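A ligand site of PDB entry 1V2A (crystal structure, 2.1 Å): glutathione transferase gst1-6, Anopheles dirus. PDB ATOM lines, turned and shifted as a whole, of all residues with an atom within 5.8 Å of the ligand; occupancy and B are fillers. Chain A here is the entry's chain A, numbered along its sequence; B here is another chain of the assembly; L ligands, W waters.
N of Ile 51 lies within hydrogen-bond range of O4 of the ligand (2.6 Å). N2 of the ligand is in hydrogen-bond range of O of Ile 51. The backbone carbonyl oxygen (O) of His 49 lies close to an oxygen (O8) of the ligand (2.8 Å). ND1 of His 49 lies within hydrogen-bond range of O8 of the ligand (2.7 Å). OG of Ser 9 sits at hydrogen-bond distance from O5 of the ligand (2.7 Å). O1 of the ligand is in hydrogen-bond range of N of Ser 64, at 2.8 Å. OG of Ser 64 lies within hydrogen-bond range of O2 of the ligand, 2.8 Å away. N1 of the ligand lies within salt-bridge range of OE1 of Glu 63, 2.9 Å away.
OG of Ser 9 is in hydrogen-bond range of SG of Cys 12, at 3.1 Å. N of Ile 100 is in hydrogen-bond range of OH of Tyr 65 (3.2 Å). The indole nitrogen (NE1) of Trp 62 sits close to the side-chain amide nitrogen (NE2) of Gln 48.
Pro 11 touches the ligand. CB of Val 33 touches C9 of the ligand, 3.7 Å away. Gln 48 touches the ligand. CA of Thr 50 touches O4 of the ligand, 2.9 Å away. CD of Pro 52 touches O1 of the ligand, 3.3 Å away. Tyr 65 touches the ligand. CD1 of Ile 100 touches N1 of the ligand, 3.9 Å away. Hydrophobic or aromatic side chains that line the ligand: Pro 11, Val 33, His 49, Ile 51, Pro 52, Tyr 65 and Ile 100.
Water W1 lies within hydrogen-bond range of the backbone carbonyl oxygen of Pro 52 (2.6 Å), the backbone NH of Glu 63 (2.7 Å), an oxygen (O1) of the ligand (2.9 Å) and the side-chain hydroxyl of Thr 50 (3.2 Å).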
ATOM      1  N   SER A   6      -6.180  17.419  -2.709  1.00  0.00           N
ATOM      2  CA  SER A   6      -5.807  17.307  -4.112  1.00  0.00           C
ATOM      3  C   SER A   6      -6.349  18.606  -4.714  1.00  0.00           C
ATOM      4  O   SER A   6      -7.538  18.875  -4.624  1.00  0.00           O
ATOM      5  CB  SER A   6      -6.480  16.095  -4.777  1.00  0.00           C
ATOM      6  OG  SER A   6      -6.089  15.981  -6.132  1.00  0.00           O
ATOM      7  N   ILE A   8      -7.077  19.462  -7.535  1.00  0.00           N
ATOM      8  CA  ILE A   8      -8.079  19.261  -8.565  1.00  0.00           C
ATOM      9  C   ILE A   8      -9.457  19.022  -7.927  1.00  0.00           C
ATOM     10  O   ILE A   8     -10.483  19.069  -8.606  1.00  0.00           O
ATOM     11  CB  ILE A   8      -7.674  18.081  -9.476  1.00  0.00           C
ATOM     12  CG1 ILE A   8      -8.666  17.925 -10.625  1.00  0.00           C
ATOM     13  CG2 ILE A   8      -7.582  16.793  -8.665  1.00  0.00           C
ATOM     14  CD1 ILE A   8      -8.230  16.914 -11.656  1.00  0.00           C
ATOM     15  N   SER A   9      -9.465  18.782  -6.622  1.00  0.00           N
ATOM     16  CA  SER A   9     -10.707  18.534  -5.906  1.00  0.00           C
ATOM     17  C   SER A   9     -11.417  19.819  -5.478  1.00  0.00           C
ATOM     18  O   SER A   9     -10.986  20.472  -4.520  1.00  0.00           O
ATOM     19  CB  SER A   9     -10.423  17.685  -4.657  1.00  0.00           C
ATOM     20  OG  SER A   9     -11.523  17.712  -3.772  1.00  0.00           O
ATOM     21  N   PRO A  10     -12.511  20.196  -6.179  1.00  0.00           N
ATOM     22  CA  PRO A  10     -13.285  21.411  -5.869  1.00  0.00           C
ATOM     23  C   PRO A  10     -13.502  21.623  -4.378  1.00  0.00           C
ATOM     24  O   PRO A  10     -13.225  22.701  -3.853  1.00  0.00           O
ATOM     25  CB  PRO A  10     -14.593  21.174  -6.625  1.00  0.00           C
ATOM     26  CG  PRO A  10     -14.081  20.510  -7.881  1.00  0.00           C
ATOM     27  CD  PRO A  10     -13.090  19.495  -7.340  1.00  0.00           C
ATOM     28  N   PRO A  11     -14.017  20.604  -3.665  1.00  0.00           N
ATOM     29  CA  PRO A  11     -14.237  20.756  -2.222  1.00  0.00           C
ATOM     30  C   PRO A  11     -12.921  21.049  -1.497  1.00  0.00           C
ATOM     31  O   PRO A  11     -12.906  21.756  -0.490  1.00  0.00           O
ATOM     32  CB  PRO A  11     -14.806  19.389  -1.813  1.00  0.00           C
ATOM     33  CG  PRO A  11     -15.505  18.935  -3.039  1.00  0.00           C
ATOM     34  CD  PRO A  11     -14.536  19.315  -4.144  1.00  0.00           C
ATOM     35  N   CYS A  12     -11.829  20.500  -2.019  1.00  0.00           N
ATOM     36  CA  CYS A  12     -10.509  20.706  -1.412  1.00  0.00           C
ATOM     37  C   CYS A  12     -10.018  22.142  -1.546  1.00  0.00           C
ATOM     38  O   CYS A  12      -9.126  22.565  -0.813  1.00  0.00           O
ATOM     39  CB  CYS A  12      -9.474  19.792  -2.069  1.00  0.00           C
ATOM     40  SG  CYS A  12      -9.511  18.081  -1.492  1.00  0.00           S
ATOM     41  N   VAL A  33      -6.433   9.292  -2.884  1.00  0.00           N
ATOM     42  CA  VAL A  33      -7.486   8.456  -2.319  1.00  0.00           C
ATOM     43  C   VAL A  33      -7.712   7.120  -3.030  1.00  0.00           C
ATOM     44  O   VAL A  33      -8.640   6.395  -2.699  1.00  0.00           O
ATOM     45  CB  VAL A  33      -8.827   9.212  -2.259  1.00  0.00           C
ATOM     46  CG1 VAL A  33      -8.690  10.430  -1.364  1.00  0.00           C
ATOM     47  CG2 VAL A  33      -9.259   9.626  -3.657  1.00  0.00           C
ATOM     48  N   GLN A  48     -14.266   7.756   6.785  1.00  0.00           N
ATOM     49  CA  GLN A  48     -14.939   7.840   5.494  1.00  0.00           C
ATOM     50  C   GLN A  48     -13.873   7.981   4.421  1.00  0.00           C
ATOM     51  O   GLN A  48     -14.146   7.871   3.223  1.00  0.00           O
ATOM     52  CB  GLN A  48     -15.903   9.025   5.436  1.00  0.00           C
ATOM     53  CG  GLN A  48     -16.817   8.979   4.207  1.00  0.00           C
ATOM     54  CD  GLN A  48     -17.917  10.014   4.211  1.00  0.00           C
ATOM     55  OE1 GLN A  48     -18.682  10.111   3.254  1.00  0.00           O
ATOM     56  NE2 GLN A  48     -18.014  10.782   5.281  1.00  0.00           N
ATOM     57  N   HIS A  49     -12.650   8.208   4.877  1.00  0.00           N
ATOM     58  CA  HIS A  49     -11.485   8.373   4.012  1.00  0.00           C
ATOM     59  C   HIS A  49     -11.746   9.203   2.768  1.00  0.00           C
ATOM     60  O   HIS A  49     -11.607   8.724   1.643  1.00  0.00           O
ATOM     61  CB  HIS A  49     -10.872   7.006   3.633  1.00  0.00           C
ATOM     62  CG  HIS A  49     -11.840   6.060   2.978  1.00  0.00           C
ATOM     63  ND1 HIS A  49     -12.316   6.249   1.697  1.00  0.00           N
ATOM     64  CD2 HIS A  49     -12.413   4.928   3.425  1.00  0.00           C
ATOM     65  CE1 HIS A  49     -13.148   5.272   1.397  1.00  0.00           C
ATOM     66  NE2 HIS A  49     -13.231   4.454   2.423  1.00  0.00           N
ATOM     67  N   THR A  50     -12.127  10.464   2.980  1.00  0.00           N
ATOM     68  CA  THR A  50     -12.377  11.386   1.882  1.00  0.00           C
ATOM     69  C   THR A  50     -11.563  12.660   2.097  1.00  0.00           C
ATOM     70  O   THR A  50     -11.199  12.988   3.229  1.00  0.00           O
ATOM     71  CB  THR A  50     -13.858  11.834   1.777  1.00  0.00           C
ATOM     72  OG1 THR A  50     -14.232  12.519   2.968  1.00  0.00           O
ATOM     73  CG2 THR A  50     -14.772  10.646   1.562  1.00  0.00           C
ATOM     74  N   ILE A  51     -11.261  13.361   1.020  1.00  0.00           N
ATOM     75  CA  ILE A  51     -10.550  14.618   1.129  1.00  0.00           C
ATOM     76  C   ILE A  51     -11.564  15.693   0.740  1.00  0.00           C
ATOM     77  O   ILE A  51     -12.445  15.466  -0.083  1.00  0.00           O
ATOM     78  CB  ILE A  51      -9.316  14.697   0.212  1.00  0.00           C
ATOM     79  CG1 ILE A  51      -9.712  14.365  -1.230  1.00  0.00           C
ATOM     80  CG2 ILE A  51      -8.234  13.768   0.721  1.00  0.00           C
ATOM     81  CD1 ILE A  51      -8.693  14.825  -2.254  1.00  0.00           C
ATOM     82  N   PRO A  52     -11.416  16.900   1.307  1.00  0.00           N
ATOM     83  CA  PRO A  52     -10.375  17.279   2.260  1.00  0.00           C
ATOM     84  C   PRO A  52     -10.537  16.690   3.657  1.00  0.00           C
ATOM     85  O   PRO A  52     -11.605  16.211   4.036  1.00  0.00           O
ATOM     86  CB  PRO A  52     -10.477  18.801   2.277  1.00  0.00           C
ATOM     87  CG  PRO A  52     -11.968  18.983   2.209  1.00  0.00           C
ATOM     88  CD  PRO A  52     -12.363  18.012   1.100  1.00  0.00           C
ATOM     89  N   TRP A  62     -13.425  16.721   8.806  1.00  0.00           N
ATOM     90  CA  TRP A  62     -13.559  16.416   7.388  1.00  0.00           C
ATOM     91  C   TRP A  62     -14.905  16.939   6.913  1.00  0.00           C
ATOM     92  O   TRP A  62     -15.786  17.209   7.737  1.00  0.00           O
ATOM     93  CB  TRP A  62     -13.325  14.925   7.092  1.00  0.00           C
ATOM     94  CG  TRP A  62     -14.407  13.985   7.447  1.00  0.00           C
ATOM     95  CD1 TRP A  62     -15.430  13.568   6.644  1.00  0.00           C
ATOM     96  CD2 TRP A  62     -14.523  13.235   8.657  1.00  0.00           C
ATOM     97  NE1 TRP A  62     -16.169  12.600   7.287  1.00  0.00           N
ATOM     98  CE2 TRP A  62     -15.635  12.386   8.523  1.00  0.00           C
ATOM     99  CE3 TRP A  62     -13.792  13.206   9.859  1.00  0.00           C
ATOM    100  CZ2 TRP A  62     -16.028  11.493   9.536  1.00  0.00           C
ATOM    101  CZ3 TRP A  62     -14.185  12.328  10.862  1.00  0.00           C
ATOM    102  CH2 TRP A  62     -15.291  11.489  10.703  1.00  0.00           C
ATOM    103  N   GLU A  63     -15.022  17.088   5.601  1.00  0.00           N
ATOM    104  CA  GLU A  63     -16.169  17.690   4.934  1.00  0.00           C
ATOM    105  C   GLU A  63     -15.722  19.156   4.812  1.00  0.00           C
ATOM    106  O   GLU A  63     -15.632  19.873   5.806  1.00  0.00           O
ATOM    107  CB  GLU A  63     -17.452  17.626   5.778  1.00  0.00           C
ATOM    108  CG  GLU A  63     -18.269  16.348   5.662  1.00  0.00           C
ATOM    109  CD  GLU A  63     -18.840  16.121   4.274  1.00  0.00           C
ATOM    110  OE1 GLU A  63     -19.224  17.118   3.613  1.00  0.00           O
ATOM    111  OE2 GLU A  63     -18.929  14.956   3.836  1.00  0.00           O
ATOM    112  N   SER A  64     -15.413  19.584   3.589  1.00  0.00           N
ATOM    113  CA  SER A  64     -14.948  20.951   3.360  1.00  0.00           C
ATOM    114  C   SER A  64     -15.724  21.967   4.195  1.00  0.00           C
ATOM    115  O   SER A  64     -15.123  22.787   4.913  1.00  0.00           O
ATOM    116  CB  SER A  64     -15.074  21.320   1.880  1.00  0.00           C
ATOM    117  OG  SER A  64     -16.428  21.276   1.440  1.00  0.00           O
ATOM    118  N   TYR A  65     -17.042  21.911   4.144  1.00  0.00           N
ATOM    119  CA  TYR A  65     -17.854  22.864   4.891  1.00  0.00           C
ATOM    120  C   TYR A  65     -17.547  22.875   6.389  1.00  0.00           C
ATOM    121  O   TYR A  65     -17.565  23.925   7.023  1.00  0.00           O
ATOM    122  CB  TYR A  65     -19.336  22.580   4.648  1.00  0.00           C
ATOM    123  CG  TYR A  65     -19.696  22.417   3.179  1.00  0.00           C
ATOM    124  CD1 TYR A  65     -19.598  21.173   2.561  1.00  0.00           C
ATOM    125  CD2 TYR A  65     -20.075  23.517   2.414  1.00  0.00           C
ATOM    126  CE1 TYR A  65     -19.870  21.035   1.198  1.00  0.00           C
ATOM    127  CE2 TYR A  65     -20.348  23.379   1.050  1.00  0.00           C
ATOM    128  CZ  TYR A  65     -20.249  22.138   0.457  1.00  0.00           C
ATOM    129  OH  TYR A  65     -20.532  21.991  -0.889  1.00  0.00           O
ATOM    130  N   ILE A 100     -23.756  21.994  -1.192  1.00  0.00           N
ATOM    131  CA  ILE A 100     -23.507  20.553  -1.194  1.00  0.00           C
ATOM    132  C   ILE A 100     -24.680  19.691  -1.631  1.00  0.00           C
ATOM    133  O   ILE A 100     -24.463  18.656  -2.274  1.00  0.00           O
ATOM    134  CB  ILE A 100     -23.068  20.059   0.221  1.00  0.00           C
ATOM    135  CG1 ILE A 100     -22.614  18.591   0.149  1.00  0.00           C
ATOM    136  CG2 ILE A 100     -24.222  20.202   1.203  1.00  0.00           C
ATOM    137  CD1 ILE A 100     -22.295  17.967   1.519  1.00  0.00           C
ATOM    138  N   TYR A 104     -23.609  22.005  -6.301  1.00  0.00           N
ATOM    139  CA  TYR A 104     -22.476  21.169  -6.629  1.00  0.00           C
ATOM    140  C   TYR A 104     -22.870  19.729  -6.942  1.00  0.00           C
ATOM    141  O   TYR A 104     -22.209  19.049  -7.727  1.00  0.00           O
ATOM    142  CB  TYR A 104     -21.457  21.167  -5.506  1.00  0.00           C
ATOM    143  CG  TYR A 104     -20.179  20.460  -5.893  1.00  0.00           C
ATOM    144  CD1 TYR A 104     -19.393  20.941  -6.939  1.00  0.00           C
ATOM    145  CD2 TYR A 104     -19.766  19.308  -5.235  1.00  0.00           C
ATOM    146  CE1 TYR A 104     -18.218  20.301  -7.304  1.00  0.00           C
ATOM    147  CE2 TYR A 104     -18.599  18.664  -5.595  1.00  0.00           C
ATOM    148  CZ  TYR A 104     -17.825  19.160  -6.629  1.00  0.00           C
ATOM    149  OH  TYR A 104     -16.654  18.538  -6.988  1.00  0.00           O
ATOM    150  N   ILE A 108     -21.443  17.945 -10.116  1.00  0.00           N
ATOM    151  CA  ILE A 108     -20.578  16.794  -9.972  1.00  0.00           C
ATOM    152  C   ILE A 108     -21.104  15.580 -10.725  1.00  0.00           C
ATOM    153  O   ILE A 108     -20.323  14.793 -11.257  1.00  0.00           O
ATOM    154  CB  ILE A 108     -20.372  16.444  -8.468  1.00  0.00           C
ATOM    155  CG1 ILE A 108     -18.874  16.388  -8.171  1.00  0.00           C
ATOM    156  CG2 ILE A 108     -21.045  15.128  -8.114  1.00  0.00           C
ATOM    157  CD1 ILE A 108     -18.061  15.579  -9.171  1.00  0.00           C
ATOM    158  N   HIS A 112     -18.898  13.666 -13.509  1.00  0.00           N
ATOM    159  CA  HIS A 112     -18.610  12.256 -13.359  1.00  0.00           C
ATOM    160  C   HIS A 112     -18.972  11.501 -14.631  1.00  0.00           C
ATOM    161  O   HIS A 112     -18.172  10.714 -15.151  1.00  0.00           O
ATOM    162  CB  HIS A 112     -19.388  11.701 -12.163  1.00  0.00           C
ATOM    163  CG  HIS A 112     -18.816  12.078 -10.830  1.00  0.00           C
ATOM    164  ND1 HIS A 112     -19.562  12.101  -9.683  1.00  0.00           N
ATOM    165  CD2 HIS A 112     -17.553  12.401 -10.466  1.00  0.00           C
ATOM    166  CE1 HIS A 112     -18.787  12.417  -8.660  1.00  0.00           C
ATOM    167  NE2 HIS A 112     -17.561  12.609  -9.107  1.00  0.00           N
ATOM    168  N   PHE B  97     -23.323  17.365   7.494  1.00  0.00           N
ATOM    169  CA  PHE B  97     -23.013  17.322   6.075  1.00  0.00           C
ATOM    170  C   PHE B  97     -22.926  15.895   5.598  1.00  0.00           C
ATOM    171  O   PHE B  97     -23.057  15.599   4.400  1.00  0.00           O
ATOM    172  CB  PHE B  97     -21.738  18.105   5.765  1.00  0.00           C
ATOM    173  CG  PHE B  97     -21.941  19.602   5.759  1.00  0.00           C
ATOM    174  CD1 PHE B  97     -21.725  20.356   6.909  1.00  0.00           C
ATOM    175  CD2 PHE B  97     -22.423  20.236   4.624  1.00  0.00           C
ATOM    176  CE1 PHE B  97     -21.993  21.730   6.934  1.00  0.00           C
ATOM    177  CE2 PHE B  97     -22.697  21.612   4.641  1.00  0.00           C
ATOM    178  CZ  PHE B  97     -22.474  22.355   5.796  1.00  0.00           C
HETATM  179  N1  LIG L   1     -18.729  16.541   0.855  1.00  0.00           N
HETATM  180  C1  LIG L   1     -17.321  16.222   0.828  1.00  0.00           C
HETATM  181  C2  LIG L   1     -16.612  17.532   1.182  1.00  0.00           C
HETATM  182  O1  LIG L   1     -15.572  17.471   1.813  1.00  0.00           O
HETATM  183  O2  LIG L   1     -17.106  18.600   0.831  1.00  0.00           O
HETATM  184  C3  LIG L   1     -16.978  15.709  -0.564  1.00  0.00           C
HETATM  185  C4  LIG L   1     -15.499  15.296  -0.708  1.00  0.00           C
HETATM  186  C5  LIG L   1     -15.280  14.206  -1.744  1.00  0.00           C
HETATM  187  O3  LIG L   1     -16.198  13.717  -2.400  1.00  0.00           O
HETATM  188  N2  LIG L   1     -14.011  13.848  -1.869  1.00  0.00           N
HETATM  189  C6  LIG L   1     -13.552  12.821  -2.809  1.00  0.00           C
HETATM  190  C7  LIG L   1     -12.931  11.720  -2.012  1.00  0.00           C
HETATM  191  O4  LIG L   1     -12.300  11.988  -0.974  1.00  0.00           O
HETATM  192  C8  LIG L   1     -12.478  13.305  -3.743  1.00  0.00           C
HETATM  193  S1  LIG L   1     -12.941  14.612  -4.898  1.00  0.00           S
HETATM  194  O5  LIG L   1     -13.416  15.791  -4.210  1.00  0.00           O
HETATM  195  O6  LIG L   1     -11.762  14.916  -5.658  1.00  0.00           O
HETATM  196  O7  LIG L   1     -13.988  14.157  -5.791  1.00  0.00           O
HETATM  197  N3  LIG L   1     -13.087  10.494  -2.502  1.00  0.00           N
HETATM  198  C9  LIG L   1     -12.505   9.376  -1.805  1.00  0.00           C
HETATM  199  C10 LIG L   1     -13.509   8.551  -1.087  1.00  0.00           C
HETATM  200  O8  LIG L   1     -13.073   7.580  -0.468  1.00  0.00           O
HETATM  201  O9  LIG L   1     -14.703   8.889  -1.164  1.00  0.00           O
HETATM  202  O   HOH W   1     -14.095  15.656   3.500  1.00  0.00           O
HETATM  203  O   HOH W   2     -21.131  14.659   0.021  1.00  0.00           O
HETATM  204  O   HOH W   3     -19.732  17.484  -1.653  1.00  0.00           O
